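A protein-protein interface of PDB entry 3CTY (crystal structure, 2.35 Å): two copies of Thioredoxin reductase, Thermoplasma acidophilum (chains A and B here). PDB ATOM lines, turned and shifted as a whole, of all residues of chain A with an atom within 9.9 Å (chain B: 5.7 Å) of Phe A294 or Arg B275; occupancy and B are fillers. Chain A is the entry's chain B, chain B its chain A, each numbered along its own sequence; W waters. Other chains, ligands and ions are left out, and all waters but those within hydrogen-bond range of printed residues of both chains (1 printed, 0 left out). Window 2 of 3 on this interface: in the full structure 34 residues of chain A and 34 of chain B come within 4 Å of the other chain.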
ATOM      1  N   ASN A  62      -7.479   2.812  18.691  1.00  0.00           N
ATOM      2  CA  ASN A  62      -6.132   2.470  18.284  1.00  0.00           C
ATOM      3  C   ASN A  62      -6.041   1.712  16.955  1.00  0.00           C
ATOM      4  O   ASN A  62      -5.066   1.011  16.706  1.00  0.00           O
ATOM      5  CB  ASN A  62      -5.433   1.685  19.391  1.00  0.00           C
ATOM      6  CG  ASN A  62      -6.219   0.463  19.828  1.00  0.00           C
ATOM      7  OD1 ASN A  62      -7.086  -0.031  19.104  1.00  0.00           O
ATOM      8  ND2 ASN A  62      -5.905  -0.042  21.005  1.00  0.00           N
ATOM      9  N   THR A 124     -11.259 -15.882  19.649  1.00  0.00           N
ATOM     10  CA  THR A 124     -11.322 -16.481  20.986  1.00  0.00           C
ATOM     11  C   THR A 124     -12.665 -16.251  21.664  1.00  0.00           C
ATOM     12  O   THR A 124     -13.450 -15.394  21.249  1.00  0.00           O
ATOM     13  CB  THR A 124     -10.252 -15.884  21.947  1.00  0.00           C
ATOM     14  OG1 THR A 124     -10.552 -14.502  22.197  1.00  0.00           O
ATOM     15  CG2 THR A 124      -8.857 -16.000  21.360  1.00  0.00           C
ATOM     16  N   ASN A 165      -6.989  -4.730  29.479  1.00  0.00           N
ATOM     17  CA  ASN A 165      -7.477  -3.683  28.583  1.00  0.00           C
ATOM     18  C   ASN A 165      -8.983  -3.798  28.367  1.00  0.00           C
ATOM     19  O   ASN A 165      -9.697  -2.795  28.399  1.00  0.00           O
ATOM     20  CB  ASN A 165      -6.770  -3.743  27.228  1.00  0.00           C
ATOM     21  CG  ASN A 165      -5.374  -3.153  27.269  1.00  0.00           C
ATOM     22  OD1 ASN A 165      -5.128  -2.175  27.970  1.00  0.00           O
ATOM     23  ND2 ASN A 165      -4.457  -3.734  26.500  1.00  0.00           N
ATOM     24  N   SER A 166      -9.455  -5.024  28.148  1.00  0.00           N
ATOM     25  CA  SER A 166     -10.876  -5.289  27.929  1.00  0.00           C
ATOM     26  C   SER A 166     -11.705  -4.882  29.140  1.00  0.00           C
ATOM     27  O   SER A 166     -12.632  -4.068  29.030  1.00  0.00           O
ATOM     28  CB  SER A 166     -11.103  -6.780  27.640  1.00  0.00           C
ATOM     29  OG  SER A 166     -10.597  -7.139  26.365  1.00  0.00           O
ATOM     30  N   GLU A 193      -3.208  -1.016  29.602  1.00  0.00           N
ATOM     31  CA  GLU A 193      -2.325   0.018  29.065  1.00  0.00           C
ATOM     32  C   GLU A 193      -2.479   1.354  29.791  1.00  0.00           C
ATOM     33  O   GLU A 193      -3.553   1.686  30.299  1.00  0.00           O
ATOM     34  CB  GLU A 193      -2.565   0.213  27.560  1.00  0.00           C
ATOM     35  CG  GLU A 193      -3.962   0.682  27.175  1.00  0.00           C
ATOM     36  CD  GLU A 193      -4.136   0.826  25.666  1.00  0.00           C
ATOM     37  OE1 GLU A 193      -3.718  -0.087  24.921  1.00  0.00           O
ATOM     38  OE2 GLU A 193      -4.702   1.845  25.223  1.00  0.00           O
ATOM     39  N   LEU A 250      -9.168 -15.262  27.963  1.00  0.00           N
ATOM     40  CA  LEU A 250      -9.668 -15.690  26.669  1.00  0.00           C
ATOM     41  C   LEU A 250      -9.219 -17.114  26.378  1.00  0.00           C
ATOM     42  O   LEU A 250      -8.189 -17.560  26.886  1.00  0.00           O
ATOM     43  CB  LEU A 250      -9.128 -14.756  25.580  1.00  0.00           C
ATOM     44  CG  LEU A 250      -9.393 -13.250  25.685  1.00  0.00           C
ATOM     45  CD1 LEU A 250      -8.462 -12.502  24.731  1.00  0.00           C
ATOM     46  CD2 LEU A 250     -10.844 -12.946  25.365  1.00  0.00           C
ATOM     47  N   TYR A 269      -3.645 -22.334  20.984  1.00  0.00           N
ATOM     48  CA  TYR A 269      -3.585 -21.387  19.863  1.00  0.00           C
ATOM     49  C   TYR A 269      -2.905 -22.018  18.653  1.00  0.00           C
ATOM     50  O   TYR A 269      -1.970 -22.780  18.805  1.00  0.00           O
ATOM     51  CB  TYR A 269      -2.814 -20.123  20.248  1.00  0.00           C
ATOM     52  CG  TYR A 269      -3.482 -19.282  21.306  1.00  0.00           C
ATOM     53  CD1 TYR A 269      -3.273 -19.533  22.659  1.00  0.00           C
ATOM     54  CD2 TYR A 269      -4.332 -18.231  20.951  1.00  0.00           C
ATOM     55  CE1 TYR A 269      -3.894 -18.758  23.640  1.00  0.00           C
ATOM     56  CE2 TYR A 269      -4.959 -17.451  21.920  1.00  0.00           C
ATOM     57  CZ  TYR A 269      -4.736 -17.721  23.265  1.00  0.00           C
ATOM     58  OH  TYR A 269      -5.366 -16.968  24.225  1.00  0.00           O
ATOM     59  N   SER A 274       5.844 -17.224   9.671  1.00  0.00           N
ATOM     60  CA  SER A 274       5.841 -15.801   9.335  1.00  0.00           C
ATOM     61  C   SER A 274       4.867 -15.476   8.205  1.00  0.00           C
ATOM     62  O   SER A 274       4.517 -14.316   7.995  1.00  0.00           O
ATOM     63  CB  SER A 274       7.251 -15.374   8.935  1.00  0.00           C
ATOM     64  OG  SER A 274       7.756 -16.216   7.906  1.00  0.00           O
ATOM     65  N   GLN A 276       1.768 -16.883   7.993  1.00  0.00           N
ATOM     66  CA  GLN A 276       0.458 -17.332   8.463  1.00  0.00           C
ATOM     67  C   GLN A 276       0.085 -18.771   8.111  1.00  0.00           C
ATOM     68  O   GLN A 276      -1.086 -19.119   8.135  1.00  0.00           O
ATOM     69  CB  GLN A 276      -0.635 -16.394   7.934  1.00  0.00           C
ATOM     70  CG  GLN A 276      -0.348 -14.911   8.155  1.00  0.00           C
ATOM     71  CD  GLN A 276      -0.233 -14.550   9.621  1.00  0.00           C
ATOM     72  OE1 GLN A 276       0.430 -13.582   9.979  1.00  0.00           O
ATOM     73  NE2 GLN A 276      -0.886 -15.327  10.477  1.00  0.00           N
ATOM     74  N   ALA A 286      -5.048 -16.624  11.131  1.00  0.00           N
ATOM     75  CA  ALA A 286      -4.712 -15.243  11.499  1.00  0.00           C
ATOM     76  C   ALA A 286      -5.657 -14.679  12.562  1.00  0.00           C
ATOM     77  O   ALA A 286      -6.824 -15.078  12.638  1.00  0.00           O
ATOM     78  CB  ALA A 286      -4.786 -14.358  10.270  1.00  0.00           C
ATOM     79  N   GLY A 287      -5.153 -13.733  13.352  1.00  0.00           N
ATOM     80  CA  GLY A 287      -5.957 -13.100  14.388  1.00  0.00           C
ATOM     81  C   GLY A 287      -5.716 -13.635  15.789  1.00  0.00           C
ATOM     82  O   GLY A 287      -4.708 -14.286  16.052  1.00  0.00           O
ATOM     83  N   ASP A 288      -6.665 -13.368  16.685  1.00  0.00           N
ATOM     84  CA  ASP A 288      -6.585 -13.801  18.083  1.00  0.00           C
ATOM     85  C   ASP A 288      -6.432 -15.317  18.250  1.00  0.00           C
ATOM     86  O   ASP A 288      -6.042 -15.791  19.315  1.00  0.00           O
ATOM     87  CB  ASP A 288      -7.832 -13.329  18.849  1.00  0.00           C
ATOM     88  CG  ASP A 288      -7.815 -11.833  19.141  1.00  0.00           C
ATOM     89  OD1 ASP A 288      -7.174 -11.076  18.380  1.00  0.00           O
ATOM     90  OD2 ASP A 288      -8.453 -11.407  20.133  1.00  0.00           O
ATOM     91  N   VAL A 289      -6.745 -16.080  17.209  1.00  0.00           N
ATOM     92  CA  VAL A 289      -6.618 -17.532  17.304  1.00  0.00           C
ATOM     93  C   VAL A 289      -5.168 -18.051  17.224  1.00  0.00           C
ATOM     94  O   VAL A 289      -4.864 -19.140  17.712  1.00  0.00           O
ATOM     95  CB  VAL A 289      -7.426 -18.225  16.192  1.00  0.00           C
ATOM     96  CG1 VAL A 289      -6.634 -18.186  14.872  1.00  0.00           C
ATOM     97  CG2 VAL A 289      -7.739 -19.657  16.598  1.00  0.00           C
ATOM     98  N   THR A 290      -4.282 -17.277  16.607  1.00  0.00           N
ATOM     99  CA  THR A 290      -2.883 -17.686  16.431  1.00  0.00           C
ATOM    100  C   THR A 290      -2.002 -17.506  17.679  1.00  0.00           C
ATOM    101  O   THR A 290      -2.096 -16.500  18.372  1.00  0.00           O
ATOM    102  CB  THR A 290      -2.226 -16.912  15.254  1.00  0.00           C
ATOM    103  OG1 THR A 290      -2.164 -15.509  15.562  1.00  0.00           O
ATOM    104  CG2 THR A 290      -3.037 -17.109  13.982  1.00  0.00           C
ATOM    105  N   SER A 291      -1.146 -18.483  17.954  1.00  0.00           N
ATOM    106  CA  SER A 291      -0.275 -18.383  19.119  1.00  0.00           C
ATOM    107  C   SER A 291       0.681 -17.219  19.001  1.00  0.00           C
ATOM    108  O   SER A 291       1.357 -17.059  17.981  1.00  0.00           O
ATOM    109  CB  SER A 291       0.517 -19.672  19.326  1.00  0.00           C
ATOM    110  OG  SER A 291       1.113 -20.099  18.121  1.00  0.00           O
ATOM    111  N   GLY A 292       0.719 -16.406  20.051  1.00  0.00           N
ATOM    112  CA  GLY A 292       1.597 -15.254  20.081  1.00  0.00           C
ATOM    113  C   GLY A 292       0.956 -13.961  19.611  1.00  0.00           C
ATOM    114  O   GLY A 292       1.577 -12.901  19.696  1.00  0.00           O
ATOM    115  N   ASN A 293      -0.284 -14.039  19.129  1.00  0.00           N
ATOM    116  CA  ASN A 293      -0.985 -12.861  18.628  1.00  0.00           C
ATOM    117  C   ASN A 293      -0.999 -11.744  19.664  1.00  0.00           C
ATOM    118  O   ASN A 293      -0.922 -12.010  20.856  1.00  0.00           O
ATOM    119  CB  ASN A 293      -2.430 -13.210  18.249  1.00  0.00           C
ATOM    120  CG  ASN A 293      -3.314 -13.420  19.464  1.00  0.00           C
ATOM    121  OD1 ASN A 293      -3.407 -14.531  20.001  1.00  0.00           O
ATOM    122  ND2 ASN A 293      -3.955 -12.346  19.918  1.00  0.00           N
ATOM    123  N   PHE A 294      -1.114 -10.497  19.203  1.00  0.00           N
ATOM    124  CA  PHE A 294      -1.128  -9.347  20.105  1.00  0.00           C
ATOM    125  C   PHE A 294      -2.531  -8.888  20.492  1.00  0.00           C
ATOM    126  O   PHE A 294      -2.713  -7.821  21.090  1.00  0.00           O
ATOM    127  CB  PHE A 294      -0.327  -8.187  19.494  1.00  0.00           C
ATOM    128  CG  PHE A 294       1.148  -8.469  19.396  1.00  0.00           C
ATOM    129  CD1 PHE A 294       1.649  -9.283  18.385  1.00  0.00           C
ATOM    130  CD2 PHE A 294       2.024  -7.979  20.359  1.00  0.00           C
ATOM    131  CE1 PHE A 294       3.011  -9.613  18.338  1.00  0.00           C
ATOM    132  CE2 PHE A 294       3.382  -8.298  20.326  1.00  0.00           C
ATOM    133  CZ  PHE A 294       3.879  -9.116  19.318  1.00  0.00           C
ATOM    134  N   ALA A 295      -3.520  -9.701  20.131  1.00  0.00           N
ATOM    135  CA  ALA A 295      -4.911  -9.449  20.471  1.00  0.00           C
ATOM    136  C   ALA A 295      -5.478  -8.059  20.165  1.00  0.00           C
ATOM    137  O   ALA A 295      -6.168  -7.475  21.007  1.00  0.00           O
ATOM    138  CB  ALA A 295      -5.119  -9.768  21.941  1.00  0.00           C
ATOM    139  N   GLN A 296      -5.207  -7.536  18.974  1.00  0.00           N
ATOM    140  CA  GLN A 296      -5.733  -6.218  18.584  1.00  0.00           C
ATOM    141  C   GLN A 296      -6.381  -6.321  17.212  1.00  0.00           C
ATOM    142  O   GLN A 296      -6.021  -7.173  16.404  1.00  0.00           O
ATOM    143  CB  GLN A 296      -4.624  -5.159  18.489  1.00  0.00           C
ATOM    144  CG  GLN A 296      -3.788  -4.952  19.733  1.00  0.00           C
ATOM    145  CD  GLN A 296      -4.591  -4.422  20.902  1.00  0.00           C
ATOM    146  OE1 GLN A 296      -5.246  -3.383  20.805  1.00  0.00           O
ATOM    147  NE2 GLN A 296      -4.532  -5.133  22.028  1.00  0.00           N
ATOM    148  N   ILE A 297      -7.334  -5.438  16.946  1.00  0.00           N
ATOM    149  CA  ILE A 297      -8.007  -5.416  15.663  1.00  0.00           C
ATOM    150  C   ILE A 297      -6.956  -5.210  14.556  1.00  0.00           C
ATOM    151  O   ILE A 297      -6.901  -5.968  13.571  1.00  0.00           O
ATOM    152  CB  ILE A 297      -9.027  -4.278  15.623  1.00  0.00           C
ATOM    153  CG1 ILE A 297     -10.107  -4.509  16.686  1.00  0.00           C
ATOM    154  CG2 ILE A 297      -9.630  -4.167  14.235  1.00  0.00           C
ATOM    155  CD1 ILE A 297     -10.945  -3.288  16.953  1.00  0.00           C
ATOM    156  N   ALA A 298      -6.121  -4.192  14.744  1.00  0.00           N
ATOM    157  CA  ALA A 298      -5.060  -3.836  13.792  1.00  0.00           C
ATOM    158  C   ALA A 298      -4.212  -5.005  13.336  1.00  0.00           C
ATOM    159  O   ALA A 298      -4.052  -5.227  12.126  1.00  0.00           O
ATOM    160  CB  ALA A 298      -4.138  -2.763  14.388  1.00  0.00           C
ATOM    161  N   SER A 299      -3.648  -5.740  14.292  1.00  0.00           N
ATOM    162  CA  SER A 299      -2.787  -6.863  13.931  1.00  0.00           C
ATOM    163  C   SER A 299      -3.612  -7.984  13.322  1.00  0.00           C
ATOM    164  O   SER A 299      -3.120  -8.754  12.492  1.00  0.00           O
ATOM    165  CB  SER A 299      -2.002  -7.380  15.144  1.00  0.00           C
ATOM    166  OG  SER A 299      -2.853  -7.941  16.126  1.00  0.00           O
ATOM    167  N   ALA A 300      -4.873  -8.066  13.729  1.00  0.00           N
ATOM    168  CA  ALA A 300      -5.758  -9.084  13.200  1.00  0.00           C
ATOM    169  C   ALA A 300      -5.968  -8.803  11.720  1.00  0.00           C
ATOM    170  O   ALA A 300      -5.855  -9.703  10.892  1.00  0.00           O
ATOM    171  CB  ALA A 300      -7.082  -9.064  13.929  1.00  0.00           C
ATOM    172  N   VAL A 301      -6.256  -7.544  11.394  1.00  0.00           N
ATOM    173  CA  VAL A 301      -6.494  -7.145  10.011  1.00  0.00           C
ATOM    174  C   VAL A 301      -5.238  -7.421   9.208  1.00  0.00           C
ATOM    175  O   VAL A 301      -5.296  -8.012   8.109  1.00  0.00           O
ATOM    176  CB  VAL A 301      -6.865  -5.647   9.915  1.00  0.00           C
ATOM    177  CG1 VAL A 301      -6.863  -5.200   8.477  1.00  0.00           C
ATOM    178  CG2 VAL A 301      -8.246  -5.416  10.513  1.00  0.00           C
ATOM    179  N   ASP A 303      -2.633  -9.534   9.809  1.00  0.00           N
ATOM    180  CA  ASP A 303      -2.374 -10.951   9.559  1.00  0.00           C
ATOM    181  C   ASP A 303      -3.411 -11.578   8.615  1.00  0.00           C
ATOM    182  O   ASP A 303      -3.085 -12.483   7.818  1.00  0.00           O
ATOM    183  CB  ASP A 303      -2.280 -11.717  10.890  1.00  0.00           C
ATOM    184  CG  ASP A 303      -1.049 -11.290  11.722  1.00  0.00           C
ATOM    185  OD1 ASP A 303      -0.256 -10.442  11.236  1.00  0.00           O
ATOM    186  OD2 ASP A 303      -0.868 -11.793  12.855  1.00  0.00           O
ATOM    187  N   LYS A 306      -2.098 -10.880   5.325  1.00  0.00           N
ATOM    188  CA  LYS A 306      -0.985 -11.778   5.010  1.00  0.00           C
ATOM    189  C   LYS A 306      -1.453 -13.189   4.651  1.00  0.00           C
ATOM    190  O   LYS A 306      -1.025 -13.760   3.647  1.00  0.00           O
ATOM    191  CB  LYS A 306      -0.010 -11.872   6.180  1.00  0.00           C
ATOM    192  CG  LYS A 306       0.604 -10.541   6.638  1.00  0.00           C
ATOM    193  CD  LYS A 306       1.783 -10.812   7.576  1.00  0.00           C
ATOM    194  CE  LYS A 306       2.252  -9.531   8.267  1.00  0.00           C
ATOM    195  NZ  LYS A 306       3.514  -9.722   9.041  1.00  0.00           N
ATOM    196  N   ASP B 273      12.168 -10.531  13.886  1.00  0.00           N
ATOM    197  CA  ASP B 273      11.576 -11.778  14.356  1.00  0.00           C
ATOM    198  C   ASP B 273      10.051 -11.645  14.357  1.00  0.00           C
ATOM    199  O   ASP B 273       9.506 -10.624  13.912  1.00  0.00           O
ATOM    200  CB  ASP B 273      12.084 -12.143  15.760  1.00  0.00           C
ATOM    201  CG  ASP B 273      11.706 -11.119  16.822  1.00  0.00           C
ATOM    202  OD1 ASP B 273      10.821 -10.275  16.576  1.00  0.00           O
ATOM    203  OD2 ASP B 273      12.297 -11.173  17.923  1.00  0.00           O
ATOM    204  N   SER B 274       9.368 -12.667  14.860  1.00  0.00           N
ATOM    205  CA  SER B 274       7.909 -12.662  14.892  1.00  0.00           C
ATOM    206  C   SER B 274       7.318 -11.566  15.770  1.00  0.00           C
ATOM    207  O   SER B 274       6.103 -11.354  15.769  1.00  0.00           O
ATOM    208  CB  SER B 274       7.380 -14.028  15.350  1.00  0.00           C
ATOM    209  OG  SER B 274       7.788 -14.325  16.674  1.00  0.00           O
ATOM    210  N   ARG B 275       8.164 -10.864  16.516  1.00  0.00           N
ATOM    211  CA  ARG B 275       7.670  -9.790  17.376  1.00  0.00           C
ATOM    212  C   ARG B 275       8.270  -8.449  16.959  1.00  0.00           C
ATOM    213  O   ARG B 275       8.424  -7.528  17.768  1.00  0.00           O
ATOM    214  CB  ARG B 275       7.962 -10.114  18.846  1.00  0.00           C
ATOM    215  CG  ARG B 275       7.383 -11.482  19.263  1.00  0.00           C
ATOM    216  CD  ARG B 275       7.556 -11.797  20.751  1.00  0.00           C
ATOM    217  NE  ARG B 275       6.484 -11.251  21.584  1.00  0.00           N
ATOM    218  CZ  ARG B 275       6.566 -10.124  22.286  1.00  0.00           C
ATOM    219  NH1 ARG B 275       7.683  -9.399  22.269  1.00  0.00           N
ATOM    220  NH2 ARG B 275       5.527  -9.722  23.014  1.00  0.00           N
ATOM    221  N   GLN B 276       8.589  -8.363  15.667  1.00  0.00           N
ATOM    222  CA  GLN B 276       9.147  -7.167  15.047  1.00  0.00           C
ATOM    223  C   GLN B 276      10.469  -6.669  15.655  1.00  0.00           C
ATOM    224  O   GLN B 276      10.804  -5.498  15.509  1.00  0.00           O
ATOM    225  CB  GLN B 276       8.119  -6.029  15.089  1.00  0.00           C
ATOM    226  CG  GLN B 276       6.700  -6.383  14.599  1.00  0.00           C
ATOM    227  CD  GLN B 276       6.664  -6.931  13.182  1.00  0.00           C
ATOM    228  OE1 GLN B 276       7.370  -6.449  12.300  1.00  0.00           O
ATOM    229  NE2 GLN B 276       5.828  -7.933  12.956  1.00  0.00           N
ATOM    230  N   ARG B 277      11.214  -7.544  16.328  1.00  0.00           N
ATOM    231  CA  ARG B 277      12.491  -7.142  16.931  1.00  0.00           C
ATOM    232  C   ARG B 277      13.642  -7.234  15.938  1.00  0.00           C
ATOM    233  O   ARG B 277      13.734  -8.200  15.180  1.00  0.00           O
ATOM    234  CB  ARG B 277      12.844  -8.027  18.127  1.00  0.00           C
ATOM    235  CG  ARG B 277      11.836  -8.051  19.251  1.00  0.00           C
ATOM    236  CD  ARG B 277      12.562  -8.228  20.575  1.00  0.00           C
ATOM    237  NE  ARG B 277      11.762  -8.895  21.599  1.00  0.00           N
ATOM    238  CZ  ARG B 277      11.445 -10.186  21.573  1.00  0.00           C
ATOM    239  NH1 ARG B 277      11.854 -10.955  20.573  1.00  0.00           N
ATOM    240  NH2 ARG B 277      10.741 -10.712  22.564  1.00  0.00           N
ATOM    241  N   TYR B 284      13.251  -1.719  16.962  1.00  0.00           N
ATOM    242  CA  TYR B 284      12.222  -2.505  16.302  1.00  0.00           C
ATOM    243  C   TYR B 284      11.950  -1.940  14.912  1.00  0.00           C
ATOM    244  O   TYR B 284      12.244  -0.779  14.649  1.00  0.00           O
ATOM    245  CB  TYR B 284      10.957  -2.465  17.152  1.00  0.00           C
ATOM    246  CG  TYR B 284      11.199  -2.865  18.594  1.00  0.00           C
ATOM    247  CD1 TYR B 284      11.033  -4.189  19.010  1.00  0.00           C
ATOM    248  CD2 TYR B 284      11.619  -1.921  19.541  1.00  0.00           C
ATOM    249  CE1 TYR B 284      11.277  -4.565  20.338  1.00  0.00           C
ATOM    250  CE2 TYR B 284      11.867  -2.286  20.865  1.00  0.00           C
ATOM    251  CZ  TYR B 284      11.692  -3.610  21.256  1.00  0.00           C
ATOM    252  OH  TYR B 284      11.919  -3.980  22.558  1.00  0.00           O
ATOM    253  N   CYS B 305       1.697  -1.964  14.800  1.00  0.00           N
ATOM    254  CA  CYS B 305       1.025  -2.183  16.078  1.00  0.00           C
ATOM    255  C   CYS B 305       1.879  -3.159  16.884  1.00  0.00           C
ATOM    256  O   CYS B 305       2.181  -2.911  18.046  1.00  0.00           O
ATOM    257  CB  CYS B 305      -0.372  -2.786  15.862  1.00  0.00           C
ATOM    258  SG  CYS B 305      -1.085  -3.722  17.301  1.00  0.00           S
ATOM    259  N   LYS B 306       2.273  -4.264  16.254  1.00  0.00           N
ATOM    260  CA  LYS B 306       3.078  -5.271  16.929  1.00  0.00           C
ATOM    261  C   LYS B 306       4.382  -4.704  17.483  1.00  0.00           C
ATOM    262  O   LYS B 306       4.693  -4.903  18.658  1.00  0.00           O
ATOM    263  CB  LYS B 306       3.395  -6.439  15.995  1.00  0.00           C
ATOM    264  CG  LYS B 306       2.188  -7.269  15.569  1.00  0.00           C
ATOM    265  CD  LYS B 306       2.617  -8.424  14.678  1.00  0.00           C
ATOM    266  CE  LYS B 306       1.430  -9.017  13.925  1.00  0.00           C
ATOM    267  NZ  LYS B 306       1.845 -10.035  12.918  1.00  0.00           N
ATOM    268  N   ALA B 307       5.140  -4.008  16.637  1.00  0.00           N
ATOM    269  CA  ALA B 307       6.404  -3.428  17.068  1.00  0.00           C
ATOM    270  C   ALA B 307       6.228  -2.622  18.357  1.00  0.00           C
ATOM    271  O   ALA B 307       6.962  -2.834  19.312  1.00  0.00           O
ATOM    272  CB  ALA B 307       6.994  -2.544  15.962  1.00  0.00           C
ATOM    273  N   LEU B 309       3.796  -2.712  20.721  1.00  0.00           N
ATOM    274  CA  LEU B 309       3.411  -3.540  21.864  1.00  0.00           C
ATOM    275  C   LEU B 309       4.572  -4.455  22.247  1.00  0.00           C
ATOM    276  O   LEU B 309       4.772  -4.769  23.419  1.00  0.00           O
ATOM    277  CB  LEU B 309       2.171  -4.379  21.529  1.00  0.00           C
ATOM    278  CG  LEU B 309       0.868  -3.603  21.289  1.00  0.00           C
ATOM    279  CD1 LEU B 309      -0.198  -4.547  20.738  1.00  0.00           C
ATOM    280  CD2 LEU B 309       0.388  -2.970  22.594  1.00  0.00           C
ATOM    281  N   SER B 310       5.337  -4.883  21.250  1.00  0.00           N
ATOM    282  CA  SER B 310       6.496  -5.737  21.492  1.00  0.00           C
ATOM    283  C   SER B 310       7.539  -4.910  22.233  1.00  0.00           C
ATOM    284  O   SER B 310       8.279  -5.422  23.070  1.00  0.00           O
ATOM    285  CB  SER B 310       7.078  -6.225  20.167  1.00  0.00           C
ATOM    286  OG  SER B 310       8.329  -6.858  20.355  1.00  0.00           O
ATOM    287  N   SER B 313       6.121  -4.552  25.823  1.00  0.00           N
ATOM    288  CA  SER B 313       6.311  -5.858  26.434  1.00  0.00           C
ATOM    289  C   SER B 313       7.712  -5.996  27.040  1.00  0.00           C
ATOM    290  O   SER B 313       7.866  -6.414  28.182  1.00  0.00           O
ATOM    291  CB  SER B 313       6.093  -6.948  25.384  1.00  0.00           C
ATOM    292  OG  SER B 313       6.698  -8.164  25.776  1.00  0.00           O
ATOM    293  N   ASP B 314       8.739  -5.642  26.280  1.00  0.00           N
ATOM    294  CA  ASP B 314      10.095  -5.753  26.795  1.00  0.00           C
ATOM    295  C   ASP B 314      10.432  -4.664  27.810  1.00  0.00           C
ATOM    296  O   ASP B 314      11.152  -4.911  28.773  1.00  0.00           O
ATOM    297  CB  ASP B 314      11.110  -5.714  25.651  1.00  0.00           C
ATOM    298  CG  ASP B 314      10.924  -6.846  24.667  1.00  0.00           C
ATOM    299  OD1 ASP B 314      10.528  -7.952  25.095  1.00  0.00           O
ATOM    300  OD2 ASP B 314      11.187  -6.632  23.466  1.00  0.00           O
HETATM  301  O   HOH W   1       2.725 -12.211  10.847  1.00  0.00           O
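Hydrophobic or aromatic side chains of chain B within 4 Å of the printed part of chain A: Leu B309.
Among the printed residues, 7 pairs touch across the chains.
Among the printed residues, Asp or Glu carboxylates within 4 Å of a Lys or Arg side-chain nitrogen of the other chain: Asp A303 with Lys B306 (2.7 Å).
Positions printed for both chains: 274, 276 and 306.
The side-chain carboxylate (OD1) of Asp B273 is in hydrogen-bond range of the backbone NH (N) of Arg B275 (2.7 Å).
The side-chain hydroxyl (OG) of Ser B310 lies within hydrogen-bond range of the backbone carbonyl oxygen (O) of Arg B275 (2.7 Å).
OG of Ser B313 sits at hydrogen-bond distance from NH2 of Arg B275, 3.4 Å away.
OD1 of Asp A303 lies close to OE1 of Gln A276, at 3.5 Å.
The backbone carbonyl oxygen of Phe A294 lies close to the side-chain amide nitrogen of Gln A296 (3.4 Å).
The backbone carbonyl oxygen (O) of Gln A296 lies within hydrogen-bond range of the side-chain hydroxyl (OG) of Ser A299.
Among the printed residues, pairs that only touch across the chains: Phe A294 with Arg B275, Phe A294 with Lys B306, Phe A294 with Leu B309, Gln A296 with Cys B305, Gln A296 with Leu B309 and Ser A299 with Lys B306.
The side-chain amino group (NZ) of Lys B306 lies within salt-bridge range of the side-chain carboxylate (OD1) of Asp A303 (2.7 Å).
Water W1 lies within hydrogen-bond range of OE1 of Gln A276, NZ of Lys B306, NZ of Lys A306 and OD1 of Asp A303.
Phe A294 touches just these residues of chain B: Arg B275, Lys B306 and Leu B309.
Gln B276 touches none of the printed residues of chain A.
No residue of chain A comes within 4 Å of Arg B277.
No residue of chain A comes within 4 Å of Ala B307.
Leu B309 touches just these residues of chain A: Phe A294 (3.8 Å) and Gln A296 (3.7 Å).
Printed residues of chain B within 4 Å of Gln A296: Cys B305 and Leu B309.
Of the printed residues of chain A, Cys B305 touches Gln A296.
Of the printed residues of chain B, Ser A299 touches Lys B306 (3.99 Å).
Printed residues of chain B within 4 Å of Asp A303: Lys B306.
Of the printed residues of chain A, Lys B306 touches Phe A294 (3.5 Å), Ser A299 (3.99 Å) and Asp A303 (2.7 Å).
Ser A166 touches none of the printed residues of chain B.
Asn A293 touches none of the printed residues of chain B.
The nearest residue of chain A that does not touch Arg B275 is Gly A292 (5.5 Å).
The nearest printed residue of chain A that does not touch Lys B306 is Lys A306 (4.2 Å).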
